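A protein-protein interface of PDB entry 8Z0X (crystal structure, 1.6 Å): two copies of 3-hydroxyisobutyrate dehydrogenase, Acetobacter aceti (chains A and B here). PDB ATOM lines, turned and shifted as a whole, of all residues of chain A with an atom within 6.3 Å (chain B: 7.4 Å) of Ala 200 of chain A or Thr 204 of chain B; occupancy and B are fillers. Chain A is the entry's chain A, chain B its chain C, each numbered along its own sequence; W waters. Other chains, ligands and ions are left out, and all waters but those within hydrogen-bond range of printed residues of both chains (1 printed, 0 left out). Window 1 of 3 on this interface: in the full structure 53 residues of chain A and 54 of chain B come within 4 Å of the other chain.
OG1 of Thr 277 of chain A sits at hydrogen-bond distance from OG1 of Thr 203 of chain B, at 2.9 Å.
N of Leu 278 of chain A sits at hydrogen-bond distance from OE1 of Glu 207 of chain B, at 3.1 Å.
The side-chain hydroxyl (OG1) of Thr 203 of chain A sits at hydrogen-bond distance from the side-chain hydroxyl (OG1) of Thr 277 of chain B, at 2.9 Å.
OE2 of Glu 207 of chain B lies within hydrogen-bond range of OG1 of Thr 277 of chain A (2.7 Å).
The side-chain amide nitrogen of Gln 284 of chain B is in hydrogen-bond range of the side-chain carboxylate of Glu 207 of chain B, 2.8 Å away.
The backbone carbonyl oxygen of Ala 200 of chain A lies within hydrogen-bond range of the side-chain hydroxyl of Thr 203 of chain A (3.3 Å).
N of Leu 202 of chain A is in hydrogen-bond range of NE2 of His 236 of chain A (3.4 Å).
The backbone carbonyl oxygen (O) of Ala 200 of chain B sits at hydrogen-bond distance from the side-chain hydroxyl (OG1) of Thr 203 of chain B, at 3.3 Å.
OG of Ser 208 of chain B sits at hydrogen-bond distance from O of Thr 204 of chain B, 2.9 Å away.
The side-chain hydroxyl (OG1) of Thr 204 of chain B sits at hydrogen-bond distance from the backbone carbonyl oxygen (O) of Ala 200 of chain B (2.8 Å).
Among the printed residues, merely in contact across the chains: Thr 204 of chain A with Ala 200 of chain B, Ala 200 of chain A with Thr 204 of chain B, Ile 197 of chain A with Ser 208 of chain B, Thr 277 of chain A with Thr 204 of chain B, Thr 204 of chain A with Thr 277 of chain B, Ile 197 of chain A with Val 231 of chain B, Thr 277 of chain A with Thr 277 of chain B, His 236 of chain A with Val 231 of chain B, Leu 278 of chain A with Ser 208 of chain B, Thr 204 of chain A with Ile 197 of chain B, Ile 197 of chain A with Thr 204 of chain B, Ala 281 of chain A with Thr 277 of chain B, Thr 277 of chain A with Ala 281 of chain B, Ile 197 of chain A with Leu 205 of chain B, Leu 205 of chain A with Ile 197 of chain B and Gly 196 of chain A with Thr 204 of chain B.
Of the printed residues of chain A, Thr 204 of chain B touches Gly 196 (3.997 Å), Ile 197 (3.7 Å), Ala 200 (3.4 Å) and Thr 277 (3.4 Å).
No residue of chain B comes within 4 Å of Gly 199 of chain A.
Printed residues of chain B within 4 Å of Ala 281 of chain A: Thr 277.
Of the printed residues of chain A, Glu 207 of chain B touches Thr 277 and Leu 278.
Printed residues of chain B within 4 Å of Leu 278 of chain A: Glu 207 and Ser 208.
Of the printed residues of chain B, Thr 277 of chain A touches Thr 203 (2.9 Å), Thr 204 (3.4 Å), Glu 207 (2.7 Å), Thr 277 (3.6 Å) and Ala 281 (3.8 Å).
Of the printed residues of chain B, Ile 197 of chain A touches Thr 204 (3.7 Å), Leu 205 (3.8 Å), Ser 208 (3.4 Å) and Val 231 (3.5 Å).
Val 209 of chain B touches none of the printed residues of chain A.
The nearest printed residue of chain A that does not touch Thr 204 of chain B is Leu 278 of chain A (4.1 Å).
The nearest printed residue of chain A that does not touch Ile 197 of chain B is Gly 201 of chain A (6.4 Å).
Hydrophobic or aromatic side chains of chain A within 4 Å of the printed part of chain B: Ile 197, Ala 200, Leu 205, His 236 and Leu 278.
Among the printed residues, 20 pairs touch across the chains.
Among the printed residues, no Asp or Glu carboxylate lies within 4 Å of a Lys or Arg side-chain nitrogen of the other chain.
Ile 197 of chain A touches Leu 205 of chain B, and with the chains exchanged Leu 205 of chain A touches Ile 197 of chain B.
Ala 200 of chain A touches Thr 204 of chain B, and with the chains exchanged Thr 204 of chain A touches Ala 200 of chain B.
Thr 204 of chain A touches Thr 277 of chain B, and with the chains exchanged Thr 277 of chain A touches Thr 204 of chain B.
Thr 277 of chain B touches its own counterpart, Thr 277 of chain A.
Positions printed for both chains: 197, 198, 199, 200, 201, 202, 203, 204, 205, 277 and 281.
Water W1 lies within hydrogen-bond range of OG1 of Thr 204 of chain A, OG1 of Thr 204 of chain B, O of Ala 200 of chain A and O of Ala 200 of chain B.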
ATOM      1  N   ASN A 195       9.681  15.560 -26.314  1.00  0.00           N
ATOM      2  CA  ASN A 195       9.586  14.179 -26.791  1.00  0.00           C
ATOM      3  C   ASN A 195       9.484  13.206 -25.624  1.00  0.00           C
ATOM      4  O   ASN A 195       8.709  12.236 -25.669  1.00  0.00           O
ATOM      5  CB  ASN A 195      10.813  13.830 -27.635  1.00  0.00           C
ATOM      6  CG  ASN A 195      10.737  14.361 -29.047  1.00  0.00           C
ATOM      7  OD1 ASN A 195       9.662  14.723 -29.546  1.00  0.00           O
ATOM      8  ND2 ASN A 195      11.888  14.388 -29.716  1.00  0.00           N
ATOM      9  N   GLY A 196      10.269  13.430 -24.575  1.00  0.00           N
ATOM     10  CA  GLY A 196      10.208  12.536 -23.433  1.00  0.00           C
ATOM     11  C   GLY A 196       8.868  12.565 -22.727  1.00  0.00           C
ATOM     12  O   GLY A 196       8.349  11.529 -22.312  1.00  0.00           O
ATOM     13  N   ILE A 197       8.293  13.755 -22.573  1.00  0.00           N
ATOM     14  CA  ILE A 197       6.971  13.874 -21.970  1.00  0.00           C
ATOM     15  C   ILE A 197       5.939  13.129 -22.805  1.00  0.00           C
ATOM     16  O   ILE A 197       5.071  12.430 -22.272  1.00  0.00           O
ATOM     17  CB  ILE A 197       6.613  15.358 -21.821  1.00  0.00           C
ATOM     18  CG1 ILE A 197       7.553  16.012 -20.819  1.00  0.00           C
ATOM     19  CG2 ILE A 197       5.157  15.534 -21.409  1.00  0.00           C
ATOM     20  CD1 ILE A 197       7.442  17.522 -20.821  1.00  0.00           C
ATOM     21  N   MET A 198       6.007  13.291 -24.131  1.00  0.00           N
ATOM     22  CA  MET A 198       5.090  12.587 -25.029  1.00  0.00           C
ATOM     23  C   MET A 198       5.237  11.076 -24.893  1.00  0.00           C
ATOM     24  O   MET A 198       4.245  10.339 -24.766  1.00  0.00           O
ATOM     25  CB  MET A 198       5.379  12.942 -26.487  1.00  0.00           C
ATOM     26  CG  MET A 198       4.348  12.355 -27.406  1.00  0.00           C
ATOM     27  SD  MET A 198       4.371  13.168 -28.996  1.00  0.00           S
ATOM     28  CE  MET A 198       5.890  12.464 -29.564  1.00  0.00           C
ATOM     29  N   GLY A 199       6.475  10.592 -25.012  1.00  0.00           N
ATOM     30  CA  GLY A 199       6.692   9.160 -25.031  1.00  0.00           C
ATOM     31  C   GLY A 199       6.278   8.503 -23.734  1.00  0.00           C
ATOM     32  O   GLY A 199       5.553   7.503 -23.727  1.00  0.00           O
ATOM     33  N   ALA A 200       6.742   9.050 -22.614  1.00  0.00           N
ATOM     34  CA  ALA A 200       6.391   8.459 -21.335  1.00  0.00           C
ATOM     35  C   ALA A 200       4.930   8.696 -20.964  1.00  0.00           C
ATOM     36  O   ALA A 200       4.353   7.906 -20.213  1.00  0.00           O
ATOM     37  CB  ALA A 200       7.332   9.003 -20.254  1.00  0.00           C
ATOM     38  N   GLY A 201       4.299   9.756 -21.490  1.00  0.00           N
ATOM     39  CA  GLY A 201       2.865   9.908 -21.297  1.00  0.00           C
ATOM     40  C   GLY A 201       2.094   8.758 -21.917  1.00  0.00           C
ATOM     41  O   GLY A 201       1.115   8.261 -21.343  1.00  0.00           O
ATOM     42  N   LEU A 202       2.545   8.300 -23.091  1.00  0.00           N
ATOM     43  CA  LEU A 202       1.865   7.195 -23.753  1.00  0.00           C
ATOM     44  C   LEU A 202       2.132   5.880 -23.029  1.00  0.00           C
ATOM     45  O   LEU A 202       1.206   5.097 -22.804  1.00  0.00           O
ATOM     46  CB  LEU A 202       2.305   7.114 -25.218  1.00  0.00           C
ATOM     47  CG  LEU A 202       1.536   6.186 -26.179  1.00  0.00           C
ATOM     48  CD1 LEU A 202       2.038   4.744 -26.063  1.00  0.00           C
ATOM     49  CD2 LEU A 202       0.014   6.260 -25.948  1.00  0.00           C
ATOM     50  N   THR A 203       3.396   5.609 -22.646  1.00  0.00           N
ATOM     51  CA  THR A 203       3.652   4.327 -21.984  1.00  0.00           C
ATOM     52  C   THR A 203       2.954   4.267 -20.629  1.00  0.00           C
ATOM     53  O   THR A 203       2.424   3.208 -20.242  1.00  0.00           O
ATOM     54  CB  THR A 203       5.164   4.054 -21.849  1.00  0.00           C
ATOM     55  OG1 THR A 203       5.741   4.955 -20.883  1.00  0.00           O
ATOM     56  CG2 THR A 203       5.870   4.243 -23.196  1.00  0.00           C
ATOM     57  N   THR A 204       2.910   5.395 -19.909  1.00  0.00           N
ATOM     58  CA  THR A 204       2.140   5.471 -18.669  1.00  0.00           C
ATOM     59  C   THR A 204       0.688   5.100 -18.906  1.00  0.00           C
ATOM     60  O   THR A 204       0.109   4.302 -18.168  1.00  0.00           O
ATOM     61  CB  THR A 204       2.213   6.886 -18.097  1.00  0.00           C
ATOM     62  OG1 THR A 204       3.543   7.146 -17.662  1.00  0.00           O
ATOM     63  CG2 THR A 204       1.235   7.079 -16.932  1.00  0.00           C
ATOM     64  N   LEU A 205       0.086   5.704 -19.928  1.00  0.00           N
ATOM     65  CA  LEU A 205      -1.318   5.448 -20.217  1.00  0.00           C
ATOM     66  C   LEU A 205      -1.549   3.996 -20.632  1.00  0.00           C
ATOM     67  O   LEU A 205      -2.488   3.349 -20.149  1.00  0.00           O
ATOM     68  CB  LEU A 205      -1.763   6.418 -21.307  1.00  0.00           C
ATOM     69  CG  LEU A 205      -3.204   6.297 -21.783  1.00  0.00           C
ATOM     70  CD1 LEU A 205      -4.170   6.486 -20.613  1.00  0.00           C
ATOM     71  CD2 LEU A 205      -3.388   7.341 -22.865  1.00  0.00           C
ATOM     72  N   HIS A 236      -2.775  12.853 -25.559  1.00  0.00           N
ATOM     73  CA  HIS A 236      -2.917  11.442 -25.248  1.00  0.00           C
ATOM     74  C   HIS A 236      -4.378  11.015 -25.162  1.00  0.00           C
ATOM     75  O   HIS A 236      -4.673   9.840 -25.395  1.00  0.00           O
ATOM     76  CB  HIS A 236      -2.147  11.126 -23.960  1.00  0.00           C
ATOM     77  CG  HIS A 236      -0.660  11.323 -24.096  1.00  0.00           C
ATOM     78  ND1 HIS A 236      -0.007  12.457 -23.648  1.00  0.00           N
ATOM     79  CD2 HIS A 236       0.295  10.531 -24.639  1.00  0.00           C
ATOM     80  CE1 HIS A 236       1.287  12.346 -23.908  1.00  0.00           C
ATOM     81  NE2 HIS A 236       1.495  11.188 -24.510  1.00  0.00           N
ATOM     82  N   MET A 257       9.552   7.682 -32.939  1.00  0.00           N
ATOM     83  CA  MET A 257       9.380   8.033 -31.532  1.00  0.00           C
ATOM     84  C   MET A 257      10.446   7.332 -30.703  1.00  0.00           C
ATOM     85  O   MET A 257      11.046   7.931 -29.808  1.00  0.00           O
ATOM     86  CB  MET A 257       7.976   7.632 -31.060  1.00  0.00           C
ATOM     87  CG  MET A 257       7.677   7.667 -29.545  1.00  0.00           C
ATOM     88  SD  MET A 257       7.329   9.311 -28.833  1.00  0.00           S
ATOM     89  CE  MET A 257       8.891  10.158 -28.639  1.00  0.00           C
ATOM     90  N   MET A 261      13.389   8.849 -28.292  1.00  0.00           N
ATOM     91  CA  MET A 261      13.660   8.469 -26.906  1.00  0.00           C
ATOM     92  C   MET A 261      15.106   8.033 -26.731  1.00  0.00           C
ATOM     93  O   MET A 261      15.735   8.384 -25.724  1.00  0.00           O
ATOM     94  CB  MET A 261      12.708   7.367 -26.421  1.00  0.00           C
ATOM     95  CG  MET A 261      11.224   7.713 -26.491  1.00  0.00           C
ATOM     96  SD  MET A 261      10.758   9.071 -25.376  1.00  0.00           S
ATOM     97  CE  MET A 261      10.868   8.295 -23.758  1.00  0.00           C
ATOM     98  N   THR A 277      11.913   7.187 -15.045  1.00  0.00           N
ATOM     99  CA  THR A 277      10.617   7.037 -15.714  1.00  0.00           C
ATOM    100  C   THR A 277      10.790   7.104 -17.224  1.00  0.00           C
ATOM    101  O   THR A 277      10.203   6.292 -17.960  1.00  0.00           O
ATOM    102  CB  THR A 277       9.621   8.115 -15.243  1.00  0.00           C
ATOM    103  OG1 THR A 277       9.611   8.181 -13.816  1.00  0.00           O
ATOM    104  CG2 THR A 277       8.205   7.777 -15.692  1.00  0.00           C
ATOM    105  N   LEU A 278      11.604   8.061 -17.704  1.00  0.00           N
ATOM    106  CA  LEU A 278      11.883   8.172 -19.135  1.00  0.00           C
ATOM    107  C   LEU A 278      12.631   6.950 -19.638  1.00  0.00           C
ATOM    108  O   LEU A 278      12.418   6.505 -20.770  1.00  0.00           O
ATOM    109  CB  LEU A 278      12.691   9.445 -19.419  1.00  0.00           C
ATOM    110  CG  LEU A 278      12.044  10.756 -18.952  1.00  0.00           C
ATOM    111  CD1 LEU A 278      12.951  11.927 -19.248  1.00  0.00           C
ATOM    112  CD2 LEU A 278      10.711  10.935 -19.639  1.00  0.00           C
ATOM    113  N   ALA A 281      10.137   4.135 -20.024  1.00  0.00           N
ATOM    114  CA  ALA A 281       9.289   4.390 -21.182  1.00  0.00           C
ATOM    115  C   ALA A 281      10.017   4.041 -22.470  1.00  0.00           C
ATOM    116  O   ALA A 281       9.416   3.491 -23.405  1.00  0.00           O
ATOM    117  CB  ALA A 281       8.856   5.859 -21.189  1.00  0.00           C
ATOM    118  N   LEU A 285       8.947   1.540 -25.539  1.00  0.00           N
ATOM    119  CA  LEU A 285       8.890   1.953 -26.934  1.00  0.00           C
ATOM    120  C   LEU A 285       9.862   1.166 -27.819  1.00  0.00           C
ATOM    121  O   LEU A 285       9.585   1.021 -29.012  1.00  0.00           O
ATOM    122  CB  LEU A 285       9.091   3.476 -27.023  1.00  0.00           C
ATOM    123  CG  LEU A 285       7.829   4.171 -26.461  1.00  0.00           C
ATOM    124  CD1 LEU A 285       8.104   5.629 -26.121  1.00  0.00           C
ATOM    125  CD2 LEU A 285       6.630   4.034 -27.410  1.00  0.00           C
ATOM    126  N   ILE B 197      -1.695   7.104 -13.693  1.00  0.00           N
ATOM    127  CA  ILE B 197      -1.521   8.138 -14.700  1.00  0.00           C
ATOM    128  C   ILE B 197      -1.061   9.436 -14.050  1.00  0.00           C
ATOM    129  O   ILE B 197      -0.180  10.140 -14.570  1.00  0.00           O
ATOM    130  CB  ILE B 197      -2.832   8.323 -15.476  1.00  0.00           C
ATOM    131  CG1 ILE B 197      -3.126   7.060 -16.285  1.00  0.00           C
ATOM    132  CG2 ILE B 197      -2.765   9.564 -16.364  1.00  0.00           C
ATOM    133  CD1 ILE B 197      -4.591   7.040 -16.809  1.00  0.00           C
ATOM    134  N   MET B 198      -1.659   9.773 -12.903  1.00  0.00           N
ATOM    135  CA  MET B 198      -1.306  11.006 -12.203  1.00  0.00           C
ATOM    136  C   MET B 198       0.124  10.961 -11.677  1.00  0.00           C
ATOM    137  O   MET B 198       0.897  11.896 -11.898  1.00  0.00           O
ATOM    138  CB  MET B 198      -2.301  11.269 -11.075  1.00  0.00           C
ATOM    139  CG  MET B 198      -2.005  12.560 -10.345  1.00  0.00           C
ATOM    140  SD  MET B 198      -3.325  12.883  -9.164  1.00  0.00           S
ATOM    141  CE  MET B 198      -2.977  11.640  -7.988  1.00  0.00           C
ATOM    142  N   GLY B 199       0.487   9.873 -10.992  1.00  0.00           N
ATOM    143  CA  GLY B 199       1.823   9.793 -10.416  1.00  0.00           C
ATOM    144  C   GLY B 199       2.922   9.795 -11.465  1.00  0.00           C
ATOM    145  O   GLY B 199       3.900  10.553 -11.369  1.00  0.00           O
ATOM    146  N   ALA B 200       2.801   8.915 -12.466  1.00  0.00           N
ATOM    147  CA  ALA B 200       3.832   8.849 -13.490  1.00  0.00           C
ATOM    148  C   ALA B 200       3.816  10.075 -14.400  1.00  0.00           C
ATOM    149  O   ALA B 200       4.862  10.446 -14.946  1.00  0.00           O
ATOM    150  CB  ALA B 200       3.696   7.556 -14.307  1.00  0.00           C
ATOM    151  N   GLY B 201       2.668  10.738 -14.554  1.00  0.00           N
ATOM    152  CA  GLY B 201       2.665  11.997 -15.275  1.00  0.00           C
ATOM    153  C   GLY B 201       3.562  13.013 -14.598  1.00  0.00           C
ATOM    154  O   GLY B 201       4.300  13.752 -15.255  1.00  0.00           O
ATOM    155  N   LEU B 202       3.545  13.025 -13.266  1.00  0.00           N
ATOM    156  CA  LEU B 202       4.373  13.989 -12.548  1.00  0.00           C
ATOM    157  C   LEU B 202       5.846  13.603 -12.614  1.00  0.00           C
ATOM    158  O   LEU B 202       6.711  14.456 -12.856  1.00  0.00           O
ATOM    159  CB  LEU B 202       3.899  14.102 -11.098  1.00  0.00           C
ATOM    160  CG  LEU B 202       4.482  15.240 -10.222  1.00  0.00           C
ATOM    161  CD1 LEU B 202       5.836  14.860  -9.609  1.00  0.00           C
ATOM    162  CD2 LEU B 202       4.619  16.562 -11.016  1.00  0.00           C
ATOM    163  N   THR B 203       6.169  12.325 -12.398  1.00  0.00           N
ATOM    164  CA  THR B 203       7.588  11.968 -12.429  1.00  0.00           C
ATOM    165  C   THR B 203       8.175  12.157 -13.822  1.00  0.00           C
ATOM    166  O   THR B 203       9.325  12.599 -13.957  1.00  0.00           O
ATOM    167  CB  THR B 203       7.820  10.531 -11.922  1.00  0.00           C
ATOM    168  OG1 THR B 203       7.288   9.571 -12.858  1.00  0.00           O
ATOM    169  CG2 THR B 203       7.149  10.312 -10.580  1.00  0.00           C
ATOM    170  N   THR B 204       7.398  11.839 -14.871  1.00  0.00           N
ATOM    171  CA  THR B 204       7.812  12.128 -16.239  1.00  0.00           C
ATOM    172  C   THR B 204       8.163  13.595 -16.408  1.00  0.00           C
ATOM    173  O   THR B 204       9.202  13.944 -16.974  1.00  0.00           O
ATOM    174  CB  THR B 204       6.689  11.752 -17.211  1.00  0.00           C
ATOM    175  OG1 THR B 204       6.514  10.336 -17.222  1.00  0.00           O
ATOM    176  CG2 THR B 204       6.998  12.256 -18.621  1.00  0.00           C
ATOM    177  N   LEU B 205       7.280  14.464 -15.932  1.00  0.00           N
ATOM    178  CA  LEU B 205       7.495  15.891 -16.080  1.00  0.00           C
ATOM    179  C   LEU B 205       8.709  16.356 -15.287  1.00  0.00           C
ATOM    180  O   LEU B 205       9.522  17.130 -15.806  1.00  0.00           O
ATOM    181  CB  LEU B 205       6.228  16.627 -15.656  1.00  0.00           C
ATOM    182  CG  LEU B 205       6.205  18.140 -15.823  1.00  0.00           C
ATOM    183  CD1 LEU B 205       6.451  18.521 -17.270  1.00  0.00           C
ATOM    184  CD2 LEU B 205       4.822  18.605 -15.343  1.00  0.00           C
ATOM    185  N   ALA B 206       8.875  15.875 -14.049  1.00  0.00           N
ATOM    186  CA  ALA B 206      10.026  16.282 -13.244  1.00  0.00           C
ATOM    187  C   ALA B 206      11.333  15.868 -13.907  1.00  0.00           C
ATOM    188  O   ALA B 206      12.303  16.636 -13.930  1.00  0.00           O
ATOM    189  CB  ALA B 206       9.911  15.693 -11.824  1.00  0.00           C
ATOM    190  N   GLU B 207      11.370  14.667 -14.495  1.00  0.00           N
ATOM    191  CA  GLU B 207      12.599  14.184 -15.114  1.00  0.00           C
ATOM    192  C   GLU B 207      12.916  14.945 -16.399  1.00  0.00           C
ATOM    193  O   GLU B 207      14.085  15.217 -16.700  1.00  0.00           O
ATOM    194  CB  GLU B 207      12.441  12.687 -15.382  1.00  0.00           C
ATOM    195  CG  GLU B 207      12.489  11.904 -14.091  1.00  0.00           C
ATOM    196  CD  GLU B 207      12.165  10.452 -14.295  1.00  0.00           C
ATOM    197  OE1 GLU B 207      12.315  10.012 -15.439  1.00  0.00           O
ATOM    198  OE2 GLU B 207      11.727   9.795 -13.324  1.00  0.00           O
ATOM    199  N   SER B 208      11.888  15.230 -17.198  1.00  0.00           N
ATOM    200  CA  SER B 208      12.094  15.953 -18.445  1.00  0.00           C
ATOM    201  C   SER B 208      12.558  17.375 -18.178  1.00  0.00           C
ATOM    202  O   SER B 208      13.478  17.862 -18.841  1.00  0.00           O
ATOM    203  CB  SER B 208      10.810  15.952 -19.268  1.00  0.00           C
ATOM    204  OG  SER B 208      10.384  14.610 -19.522  1.00  0.00           O
ATOM    205  N   VAL B 209      11.925  18.050 -17.208  1.00  0.00           N
ATOM    206  CA  VAL B 209      12.403  19.365 -16.784  1.00  0.00           C
ATOM    207  C   VAL B 209      13.848  19.288 -16.313  1.00  0.00           C
ATOM    208  O   VAL B 209      14.683  20.116 -16.688  1.00  0.00           O
ATOM    209  CB  VAL B 209      11.484  19.929 -15.691  1.00  0.00           C
ATOM    210  CG1 VAL B 209      12.126  21.140 -15.020  1.00  0.00           C
ATOM    211  CG2 VAL B 209      10.135  20.305 -16.296  1.00  0.00           C
ATOM    212  N   ALA B 210      14.178  18.267 -15.521  1.00  0.00           N
ATOM    213  CA  ALA B 210      15.545  18.135 -15.030  1.00  0.00           C
ATOM    214  C   ALA B 210      16.541  17.991 -16.172  1.00  0.00           C
ATOM    215  O   ALA B 210      17.613  18.610 -16.140  1.00  0.00           O
ATOM    216  CB  ALA B 210      15.643  16.949 -14.074  1.00  0.00           C
ATOM    217  N   VAL B 231       0.998  18.006 -24.826  1.00  0.00           N
ATOM    218  CA  VAL B 231       1.311  16.672 -24.327  1.00  0.00           C
ATOM    219  C   VAL B 231       1.393  16.626 -22.804  1.00  0.00           C
ATOM    220  O   VAL B 231       1.789  15.601 -22.253  1.00  0.00           O
ATOM    221  CB  VAL B 231       2.602  16.129 -24.954  1.00  0.00           C
ATOM    222  CG1 VAL B 231       2.394  15.899 -26.453  1.00  0.00           C
ATOM    223  CG2 VAL B 231       3.777  17.069 -24.703  1.00  0.00           C
ATOM    224  N   THR B 277       7.007   1.608 -16.552  1.00  0.00           N
ATOM    225  CA  THR B 277       6.956   3.061 -16.359  1.00  0.00           C
ATOM    226  C   THR B 277       6.329   3.401 -15.013  1.00  0.00           C
ATOM    227  O   THR B 277       6.828   4.275 -14.292  1.00  0.00           O
ATOM    228  CB  THR B 277       6.173   3.741 -17.491  1.00  0.00           C
ATOM    229  OG1 THR B 277       6.620   3.228 -18.754  1.00  0.00           O
ATOM    230  CG2 THR B 277       6.398   5.253 -17.472  1.00  0.00           C
ATOM    231  N   ALA B 281       8.137   5.273 -11.779  1.00  0.00           N
ATOM    232  CA  ALA B 281       7.510   6.437 -11.160  1.00  0.00           C
ATOM    233  C   ALA B 281       7.337   6.238  -9.658  1.00  0.00           C
ATOM    234  O   ALA B 281       7.533   7.176  -8.867  1.00  0.00           O
ATOM    235  CB  ALA B 281       6.155   6.702 -11.817  1.00  0.00           C
ATOM    236  N   GLN B 284      10.526   6.942  -7.786  1.00  0.00           N
ATOM    237  CA  GLN B 284      10.746   8.381  -7.681  1.00  0.00           C
ATOM    238  C   GLN B 284       9.851   9.012  -6.623  1.00  0.00           C
ATOM    239  O   GLN B 284      10.275   9.941  -5.918  1.00  0.00           O
ATOM    240  CB  GLN B 284      10.518   9.027  -9.045  1.00  0.00           C
ATOM    241  CG  GLN B 284      11.597   8.684 -10.058  1.00  0.00           C
ATOM    242  CD  GLN B 284      12.772   9.621  -9.932  1.00  0.00           C
ATOM    243  OE1 GLN B 284      13.561   9.517  -9.005  1.00  0.00           O
ATOM    244  NE2 GLN B 284      12.887  10.546 -10.861  1.00  0.00           N
ATOM    245  N   LEU B 300       8.634  16.594  -6.233  1.00  0.00           N
ATOM    246  CA  LEU B 300       9.691  15.919  -6.980  1.00  0.00           C
ATOM    247  C   LEU B 300      10.327  16.837  -8.022  1.00  0.00           C
ATOM    248  O   LEU B 300      11.507  16.677  -8.348  1.00  0.00           O
ATOM    249  CB  LEU B 300       9.123  14.663  -7.650  1.00  0.00           C
ATOM    250  CG  LEU B 300      10.112  13.905  -8.539  1.00  0.00           C
ATOM    251  CD1 LEU B 300      11.298  13.362  -7.700  1.00  0.00           C
ATOM    252  CD2 LEU B 300       9.384  12.738  -9.161  1.00  0.00           C
HETATM  253  O   HOH W   1       3.309  10.284 -17.990  1.00  0.00           O
